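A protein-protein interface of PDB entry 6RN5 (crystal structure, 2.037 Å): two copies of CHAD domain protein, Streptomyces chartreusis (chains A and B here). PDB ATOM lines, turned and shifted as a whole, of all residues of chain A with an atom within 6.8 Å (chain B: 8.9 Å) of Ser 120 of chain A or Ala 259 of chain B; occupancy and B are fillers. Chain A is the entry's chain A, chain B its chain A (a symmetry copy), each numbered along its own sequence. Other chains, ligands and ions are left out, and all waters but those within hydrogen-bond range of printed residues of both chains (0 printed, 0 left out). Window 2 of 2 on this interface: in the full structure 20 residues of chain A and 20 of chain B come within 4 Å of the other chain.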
ATOM      1  N   ALA A 115      -0.524  -9.481  -4.125  1.00  0.00           N
ATOM      2  CA  ALA A 115       0.133  -8.200  -4.247  1.00  0.00           C
ATOM      3  C   ALA A 115       1.547  -8.235  -3.675  1.00  0.00           C
ATOM      4  O   ALA A 115       2.458  -7.697  -4.278  1.00  0.00           O
ATOM      5  CB  ALA A 115      -0.705  -7.102  -3.616  1.00  0.00           C
ATOM      6  N   LEU A 116       1.744  -8.893  -2.535  1.00  0.00           N
ATOM      7  CA  LEU A 116       3.085  -9.039  -1.941  1.00  0.00           C
ATOM      8  C   LEU A 116       4.114  -9.812  -2.804  1.00  0.00           C
ATOM      9  O   LEU A 116       5.330  -9.508  -2.790  1.00  0.00           O
ATOM     10  CB  LEU A 116       2.996  -9.759  -0.589  1.00  0.00           C
ATOM     11  CG  LEU A 116       2.524  -8.973   0.643  1.00  0.00           C
ATOM     12  CD1 LEU A 116       2.279  -9.969   1.759  1.00  0.00           C
ATOM     13  CD2 LEU A 116       3.511  -7.894   1.085  1.00  0.00           C
ATOM     14  N   HIS A 117       3.625 -10.853  -3.460  1.00  0.00           N
ATOM     15  CA  HIS A 117       4.424 -11.662  -4.368  1.00  0.00           C
ATOM     16  C   HIS A 117       4.876 -10.763  -5.504  1.00  0.00           C
ATOM     17  O   HIS A 117       6.070 -10.679  -5.797  1.00  0.00           O
ATOM     18  CB  HIS A 117       3.628 -12.867  -4.922  1.00  0.00           C
ATOM     19  CG  HIS A 117       3.645 -14.090  -4.040  1.00  0.00           C
ATOM     20  ND1 HIS A 117       4.791 -14.566  -3.430  1.00  0.00           N
ATOM     21  CD2 HIS A 117       2.656 -14.960  -3.702  1.00  0.00           C
ATOM     22  CE1 HIS A 117       4.503 -15.656  -2.734  1.00  0.00           C
ATOM     23  NE2 HIS A 117       3.216 -15.921  -2.888  1.00  0.00           N
ATOM     24  N   ARG A 118       3.916 -10.050  -6.079  1.00  0.00           N
ATOM     25  CA  ARG A 118       4.179  -9.057  -7.125  1.00  0.00           C
ATOM     26  C   ARG A 118       5.169  -7.984  -6.683  1.00  0.00           C
ATOM     27  O   ARG A 118       6.167  -7.699  -7.363  1.00  0.00           O
ATOM     28  CB  ARG A 118       2.857  -8.430  -7.547  1.00  0.00           C
ATOM     29  CG  ARG A 118       2.987  -7.231  -8.445  1.00  0.00           C
ATOM     30  CD  ARG A 118       1.684  -6.929  -9.153  1.00  0.00           C
ATOM     31  NE  ARG A 118       0.576  -6.605  -8.248  1.00  0.00           N
ATOM     32  CZ  ARG A 118       0.472  -5.488  -7.520  1.00  0.00           C
ATOM     33  NH1 ARG A 118       1.425  -4.549  -7.558  1.00  0.00           N
ATOM     34  NH2 ARG A 118      -0.607  -5.305  -6.753  1.00  0.00           N
ATOM     35  N   LEU A 119       4.916  -7.391  -5.529  1.00  0.00           N
ATOM     36  CA  LEU A 119       5.767  -6.322  -5.032  1.00  0.00           C
ATOM     37  C   LEU A 119       7.180  -6.783  -4.602  1.00  0.00           C
ATOM     38  O   LEU A 119       8.082  -5.947  -4.383  1.00  0.00           O
ATOM     39  CB  LEU A 119       5.096  -5.643  -3.841  1.00  0.00           C
ATOM     40  CG  LEU A 119       3.808  -4.920  -4.170  1.00  0.00           C
ATOM     41  CD1 LEU A 119       2.986  -4.698  -2.901  1.00  0.00           C
ATOM     42  CD2 LEU A 119       4.132  -3.620  -4.882  1.00  0.00           C
ATOM     43  N   SER A 120       7.376  -8.083  -4.443  1.00  0.00           N
ATOM     44  CA  SER A 120       8.718  -8.588  -4.209  1.00  0.00           C
ATOM     45  C   SER A 120       9.458  -8.630  -5.550  1.00  0.00           C
ATOM     46  O   SER A 120      10.576  -8.119  -5.659  1.00  0.00           O
ATOM     47  CB  SER A 120       8.666  -9.937  -3.512  1.00  0.00           C
ATOM     48  OG  SER A 120       8.152  -9.748  -2.203  1.00  0.00           O
ATOM     49  N   GLY A 121       8.804  -9.179  -6.577  1.00  0.00           N
ATOM     50  CA  GLY A 121       9.310  -9.116  -7.958  1.00  0.00           C
ATOM     51  C   GLY A 121       9.886 -10.447  -8.379  1.00  0.00           C
ATOM     52  O   GLY A 121       9.427 -11.489  -7.912  1.00  0.00           O
ATOM     53  N   LEU A 168      10.274 -14.418  -1.445  1.00  0.00           N
ATOM     54  CA  LEU A 168       9.999 -13.242  -0.621  1.00  0.00           C
ATOM     55  C   LEU A 168      11.136 -12.927   0.344  1.00  0.00           C
ATOM     56  O   LEU A 168      11.639 -13.793   1.044  1.00  0.00           O
ATOM     57  CB  LEU A 168       8.731 -13.467   0.195  1.00  0.00           C
ATOM     58  CG  LEU A 168       7.473 -13.883  -0.569  1.00  0.00           C
ATOM     59  CD1 LEU A 168       6.333 -14.130   0.409  1.00  0.00           C
ATOM     60  CD2 LEU A 168       7.104 -12.827  -1.607  1.00  0.00           C
ATOM     61  N   THR A 169      11.534 -11.677   0.392  1.00  0.00           N
ATOM     62  CA  THR A 169      12.453 -11.240   1.416  1.00  0.00           C
ATOM     63  C   THR A 169      11.761 -11.441   2.777  1.00  0.00           C
ATOM     64  O   THR A 169      10.549 -11.587   2.836  1.00  0.00           O
ATOM     65  CB  THR A 169      12.885  -9.780   1.146  1.00  0.00           C
ATOM     66  OG1 THR A 169      14.000  -9.424   1.981  1.00  0.00           O
ATOM     67  CG2 THR A 169      11.726  -8.815   1.353  1.00  0.00           C
ATOM     68  N   ALA A 172       8.475  -9.189   3.492  1.00  0.00           N
ATOM     69  CA  ALA A 172       7.346  -9.629   2.744  1.00  0.00           C
ATOM     70  C   ALA A 172       6.793 -10.945   3.257  1.00  0.00           C
ATOM     71  O   ALA A 172       5.573 -11.132   3.272  1.00  0.00           O
ATOM     72  CB  ALA A 172       7.748  -9.815   1.295  1.00  0.00           C
ATOM     73  N   ALA A 173       7.704 -11.857   3.600  1.00  0.00           N
ATOM     74  CA  ALA A 173       7.354 -13.198   4.030  1.00  0.00           C
ATOM     75  C   ALA A 173       6.662 -13.116   5.355  1.00  0.00           C
ATOM     76  O   ALA A 173       5.635 -13.763   5.559  1.00  0.00           O
ATOM     77  CB  ALA A 173       8.577 -14.083   4.145  1.00  0.00           C
ATOM     78  N   ALA B 258       9.019  -4.015 -10.181  1.00  0.00           N
ATOM     79  CA  ALA B 258       9.616  -2.839  -9.546  1.00  0.00           C
ATOM     80  C   ALA B 258      10.604  -3.186  -8.397  1.00  0.00           C
ATOM     81  O   ALA B 258      11.557  -2.428  -8.153  1.00  0.00           O
ATOM     82  CB  ALA B 258       8.507  -1.902  -9.056  1.00  0.00           C
ATOM     83  N   ALA B 259      10.393  -4.315  -7.711  1.00  0.00           N
ATOM     84  CA  ALA B 259      11.138  -4.674  -6.477  1.00  0.00           C
ATOM     85  C   ALA B 259      11.069  -3.601  -5.372  1.00  0.00           C
ATOM     86  O   ALA B 259      12.068  -2.991  -4.930  1.00  0.00           O
ATOM     87  CB  ALA B 259      12.573  -5.043  -6.783  1.00  0.00           C
ATOM     88  N   LEU B 260       9.862  -3.403  -4.903  1.00  0.00           N
ATOM     89  CA  LEU B 260       9.591  -2.428  -3.871  1.00  0.00           C
ATOM     90  C   LEU B 260       9.808  -2.971  -2.462  1.00  0.00           C
ATOM     91  O   LEU B 260      10.065  -2.218  -1.531  1.00  0.00           O
ATOM     92  CB  LEU B 260       8.182  -1.896  -4.053  1.00  0.00           C
ATOM     93  CG  LEU B 260       7.969  -1.319  -5.446  1.00  0.00           C
ATOM     94  CD1 LEU B 260       6.518  -0.933  -5.659  1.00  0.00           C
ATOM     95  CD2 LEU B 260       8.871  -0.116  -5.665  1.00  0.00           C
ATOM     96  N   ILE B 261       9.756  -4.271  -2.292  1.00  0.00           N
ATOM     97  CA  ILE B 261      10.132  -4.845  -1.023  1.00  0.00           C
ATOM     98  C   ILE B 261      11.280  -5.769  -1.341  1.00  0.00           C
ATOM     99  O   ILE B 261      11.118  -6.708  -2.104  1.00  0.00           O
ATOM    100  CB  ILE B 261       8.982  -5.640  -0.380  1.00  0.00           C
ATOM    101  CG1 ILE B 261       7.684  -4.838  -0.355  1.00  0.00           C
ATOM    102  CG2 ILE B 261       9.353  -5.979   1.051  1.00  0.00           C
ATOM    103  CD1 ILE B 261       6.455  -5.673   0.000  1.00  0.00           C
ATOM    104  N   HIS B 262      12.453  -5.437  -0.826  1.00  0.00           N
ATOM    105  CA  HIS B 262      13.662  -6.257  -0.989  1.00  0.00           C
ATOM    106  C   HIS B 262      14.473  -6.024   0.261  1.00  0.00           C
ATOM    107  O   HIS B 262      14.261  -5.001   0.948  1.00  0.00           O
ATOM    108  CB  HIS B 262      14.479  -5.865  -2.250  1.00  0.00           C
ATOM    109  CG  HIS B 262      15.028  -4.469  -2.213  1.00  0.00           C
ATOM    110  ND1 HIS B 262      16.013  -4.073  -1.334  1.00  0.00           N
ATOM    111  CD2 HIS B 262      14.682  -3.361  -2.908  1.00  0.00           C
ATOM    112  CE1 HIS B 262      16.273  -2.793  -1.511  1.00  0.00           C
ATOM    113  NE2 HIS B 262      15.478  -2.336  -2.463  1.00  0.00           N
ATOM    114  N   GLY B 263      15.374  -6.962   0.568  1.00  0.00           N
ATOM    115  CA  GLY B 263      16.335  -6.790   1.669  1.00  0.00           C
ATOM    116  C   GLY B 263      17.593  -6.038   1.237  1.00  0.00           C
ATOM    117  O   GLY B 263      17.681  -5.525   0.112  1.00  0.00           O
ATOM    118  N   THR B 268      23.460  -8.035  -2.554  1.00  0.00           N
ATOM    119  CA  THR B 268      22.195  -7.657  -3.198  1.00  0.00           C
ATOM    120  C   THR B 268      22.483  -6.643  -4.322  1.00  0.00           C
ATOM    121  O   THR B 268      23.170  -5.642  -4.090  1.00  0.00           O
ATOM    122  CB  THR B 268      21.189  -7.024  -2.178  1.00  0.00           C
ATOM    123  OG1 THR B 268      21.228  -7.735  -0.935  1.00  0.00           O
ATOM    124  CG2 THR B 268      19.740  -7.037  -2.697  1.00  0.00           C
ATOM    125  N   VAL B 269      22.007  -6.919  -5.539  1.00  0.00           N
ATOM    126  CA  VAL B 269      21.821  -5.855  -6.523  1.00  0.00           C
ATOM    127  C   VAL B 269      20.323  -5.570  -6.576  1.00  0.00           C
ATOM    128  O   VAL B 269      19.616  -6.150  -7.396  1.00  0.00           O
ATOM    129  CB  VAL B 269      22.299  -6.242  -7.927  1.00  0.00           C
ATOM    130  CG1 VAL B 269      22.190  -5.026  -8.845  1.00  0.00           C
ATOM    131  CG2 VAL B 269      23.726  -6.788  -7.887  1.00  0.00           C
ATOM    132  N   PRO B 270      19.821  -4.689  -5.690  1.00  0.00           N
ATOM    133  CA  PRO B 270      18.359  -4.573  -5.601  1.00  0.00           C
ATOM    134  C   PRO B 270      17.691  -3.937  -6.847  1.00  0.00           C
ATOM    135  O   PRO B 270      16.611  -4.358  -7.232  1.00  0.00           O
ATOM    136  CB  PRO B 270      18.152  -3.759  -4.311  1.00  0.00           C
ATOM    137  CG  PRO B 270      19.404  -2.965  -4.158  1.00  0.00           C
ATOM    138  CD  PRO B 270      20.513  -3.782  -4.747  1.00  0.00           C
ATOM    139  N   HIS B 271      18.374  -3.008  -7.516  1.00  0.00           N
ATOM    140  CA  HIS B 271      17.799  -2.253  -8.639  1.00  0.00           C
ATOM    141  C   HIS B 271      18.784  -2.277  -9.804  1.00  0.00           C
ATOM    142  O   HIS B 271      19.437  -1.292 -10.089  1.00  0.00           O
ATOM    143  CB  HIS B 271      17.484  -0.826  -8.150  1.00  0.00           C
ATOM    144  CG  HIS B 271      16.480  -0.810  -7.036  1.00  0.00           C
ATOM    145  ND1 HIS B 271      15.169  -1.182  -7.233  1.00  0.00           N
ATOM    146  CD2 HIS B 271      16.597  -0.545  -5.717  1.00  0.00           C
ATOM    147  CE1 HIS B 271      14.510  -1.117  -6.092  1.00  0.00           C
ATOM    148  NE2 HIS B 271      15.351  -0.741  -5.147  1.00  0.00           N
ATOM    149  N   PRO B 272      18.882  -3.436 -10.486  1.00  0.00           N
ATOM    150  CA  PRO B 272      19.952  -3.683 -11.451  1.00  0.00           C
ATOM    151  C   PRO B 272      19.893  -2.792 -12.673  1.00  0.00           C
ATOM    152  O   PRO B 272      20.933  -2.350 -13.152  1.00  0.00           O
ATOM    153  CB  PRO B 272      19.745  -5.163 -11.839  1.00  0.00           C
ATOM    154  CG  PRO B 272      18.331  -5.495 -11.422  1.00  0.00           C
ATOM    155  CD  PRO B 272      18.084  -4.655 -10.221  1.00  0.00           C
ATOM    156  N   ALA B 324      15.840   6.706  -2.556  1.00  0.00           N
ATOM    157  CA  ALA B 324      15.126   5.496  -2.204  1.00  0.00           C
ATOM    158  C   ALA B 324      16.027   4.607  -1.346  1.00  0.00           C
ATOM    159  O   ALA B 324      15.546   3.996  -0.399  1.00  0.00           O
ATOM    160  CB  ALA B 324      14.643   4.766  -3.446  1.00  0.00           C
ATOM    161  N   ALA B 328      15.460   2.990   2.435  1.00  0.00           N
ATOM    162  CA  ALA B 328      15.559   1.562   2.727  1.00  0.00           C
ATOM    163  C   ALA B 328      16.568   1.326   3.858  1.00  0.00           C
ATOM    164  O   ALA B 328      16.274   0.639   4.844  1.00  0.00           O
ATOM    165  CB  ALA B 328      15.915   0.736   1.468  1.00  0.00           C
ATOM    166  N   GLY B 345       9.002   2.554   4.276  1.00  0.00           N
ATOM    167  CA  GLY B 345       8.553   1.698   3.151  1.00  0.00           C
ATOM    168  C   GLY B 345       7.816   2.446   2.035  1.00  0.00           C
ATOM    169  O   GLY B 345       8.059   2.213   0.847  1.00  0.00           O
ATOM    170  N   HIS B 348      10.424   4.857   0.256  1.00  0.00           N
ATOM    171  CA  HIS B 348      11.213   4.106  -0.712  1.00  0.00           C
ATOM    172  C   HIS B 348      10.431   3.832  -1.974  1.00  0.00           C
ATOM    173  O   HIS B 348      10.961   3.997  -3.069  1.00  0.00           O
ATOM    174  CB  HIS B 348      11.709   2.790  -0.104  1.00  0.00           C
ATOM    175  CG  HIS B 348      12.339   1.861  -1.101  1.00  0.00           C
ATOM    176  ND1 HIS B 348      11.613   0.910  -1.785  1.00  0.00           N
ATOM    177  CD2 HIS B 348      13.622   1.749  -1.534  1.00  0.00           C
ATOM    178  CE1 HIS B 348      12.435   0.239  -2.589  1.00  0.00           C
ATOM    179  NE2 HIS B 348      13.656   0.741  -2.460  1.00  0.00           N
ATOM    180  N   ALA B 349       9.166   3.443  -1.834  1.00  0.00           N
ATOM    181  CA  ALA B 349       8.334   3.135  -2.972  1.00  0.00           C
ATOM    182  C   ALA B 349       8.071   4.381  -3.819  1.00  0.00           C
ATOM    183  O   ALA B 349       8.219   4.370  -5.063  1.00  0.00           O
ATOM    184  CB  ALA B 349       7.009   2.531  -2.494  1.00  0.00           C
ATOM    185  N   ARG B 352      11.129   5.158  -5.774  1.00  0.00           N
ATOM    186  CA  ARG B 352      11.267   4.229  -6.892  1.00  0.00           C
ATOM    187  C   ARG B 352      10.268   4.557  -7.999  1.00  0.00           C
ATOM    188  O   ARG B 352      10.578   4.399  -9.192  1.00  0.00           O
ATOM    189  CB  ARG B 352      11.100   2.781  -6.448  1.00  0.00           C
ATOM    190  CG  ARG B 352      12.201   2.278  -5.567  1.00  0.00           C
ATOM    191  CD  ARG B 352      13.581   2.515  -6.177  1.00  0.00           C
ATOM    192  NE  ARG B 352      13.789   1.980  -7.534  1.00  0.00           N
ATOM    193  CZ  ARG B 352      14.933   2.076  -8.221  1.00  0.00           C
ATOM    194  NH1 ARG B 352      15.994   2.705  -7.719  1.00  0.00           N
ATOM    195  NH2 ARG B 352      15.034   1.531  -9.421  1.00  0.00           N
ATOM    196  N   HIS B 353       9.089   5.070  -7.622  1.00  0.00           N
ATOM    197  CA  HIS B 353       8.133   5.562  -8.630  1.00  0.00           C
ATOM    198  C   HIS B 353       8.679   6.766  -9.368  1.00  0.00           C
ATOM    199  O   HIS B 353       8.452   6.875 -10.556  1.00  0.00           O
ATOM    200  CB  HIS B 353       6.712   5.825  -8.051  1.00  0.00           C
ATOM    201  CG  HIS B 353       6.090   4.607  -7.443  1.00  0.00           C
ATOM    202  ND1 HIS B 353       6.369   3.329  -7.890  1.00  0.00           N
ATOM    203  CD2 HIS B 353       5.228   4.460  -6.399  1.00  0.00           C
ATOM    204  CE1 HIS B 353       5.702   2.450  -7.157  1.00  0.00           C
ATOM    205  NE2 HIS B 353       4.998   3.109  -6.252  1.00  0.00           N
ATOM    206  N   GLU B 356      11.207   5.479 -12.113  1.00  0.00           N
ATOM    207  CA  GLU B 356      10.425   5.132 -13.289  1.00  0.00           C
ATOM    208  C   GLU B 356       9.887   6.347 -14.045  1.00  0.00           C
ATOM    209  O   GLU B 356      10.039   6.432 -15.248  1.00  0.00           O
ATOM    210  CB  GLU B 356       9.266   4.193 -12.922  1.00  0.00           C
ATOM    211  CG  GLU B 356       9.651   2.703 -12.950  1.00  0.00           C
ATOM    212  CD  GLU B 356      10.012   2.175 -14.361  1.00  0.00           C
ATOM    213  OE1 GLU B 356       9.231   2.349 -15.330  1.00  0.00           O
ATOM    214  OE2 GLU B 356      11.093   1.568 -14.522  1.00  0.00           O
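Among the printed residues, pairs that only touch across the chains: Ser 120 of chain A with Ala 259 of chain B, Ser 120 of chain A with Ile 261 of chain B, Thr 169 of chain A with Ile 261 of chain B, Thr 169 of chain A with His 262 of chain B, Leu 116 of chain A with Ile 261 of chain B and Leu 119 of chain A with Ala 259 of chain B.
No residue of chain B comes within 4 Å of Gly 121 of chain A. Of the printed residues of chain B, Thr 169 of chain A touches Ile 261 (3.7 Å), His 262 (3.8 Å) and Gly 263 (3.2 Å). Of the printed residues of chain B, Leu 119 of chain A touches Ala 259 (3.9 Å), Leu 260 (3.1 Å) and Ile 261 (3.2 Å). Printed residues of chain A within 4 Å of Leu 260 of chain B: Leu 119. Val 269 of chain B touches none of the printed residues of chain A. The nearest residue of chain A that does not touch Ala 259 of chain B is Gly 121 of chain A (4.9 Å).
No position is printed for both chains.
Hydrophobic or aromatic side chains of chain B within 4 Å of the printed part of chain A: Ala 259, Leu 260 and Ile 261. Hydrophobic or aromatic side chains of chain A that line the printed part of chain B: Leu 116 and Leu 119. Along chain A the printed residues that touch a printed residue of chain B span positions 116 to 169. Among the printed residues, 9 pairs touch across the chains. Among the printed residues, no Asp or Glu carboxylate lies within 4 Å of a Lys or Arg side-chain nitrogen of the other chain.
The backbone carbonyl oxygen (O) of Leu 119 of chain A is in hydrogen-bond range of the backbone NH (N) of Leu 260 of chain B (3.1 Å). The backbone carbonyl oxygen (O) of Leu 119 of chain A lies within hydrogen-bond range of the backbone NH (N) of Ile 261 of chain B (3.2 Å). The side-chain hydroxyl (OG1) of Thr 169 of chain A is in hydrogen-bond range of the backbone NH (N) of Gly 263 of chain B, at 3.2 Å.
OG of Ser 120 of chain A is in hydrogen-bond range of O of Leu 116 of chain A (2.9 Å). O of Leu 260 of chain B lies within hydrogen-bond range of ND1 of His 348 of chain B (3.5 Å).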
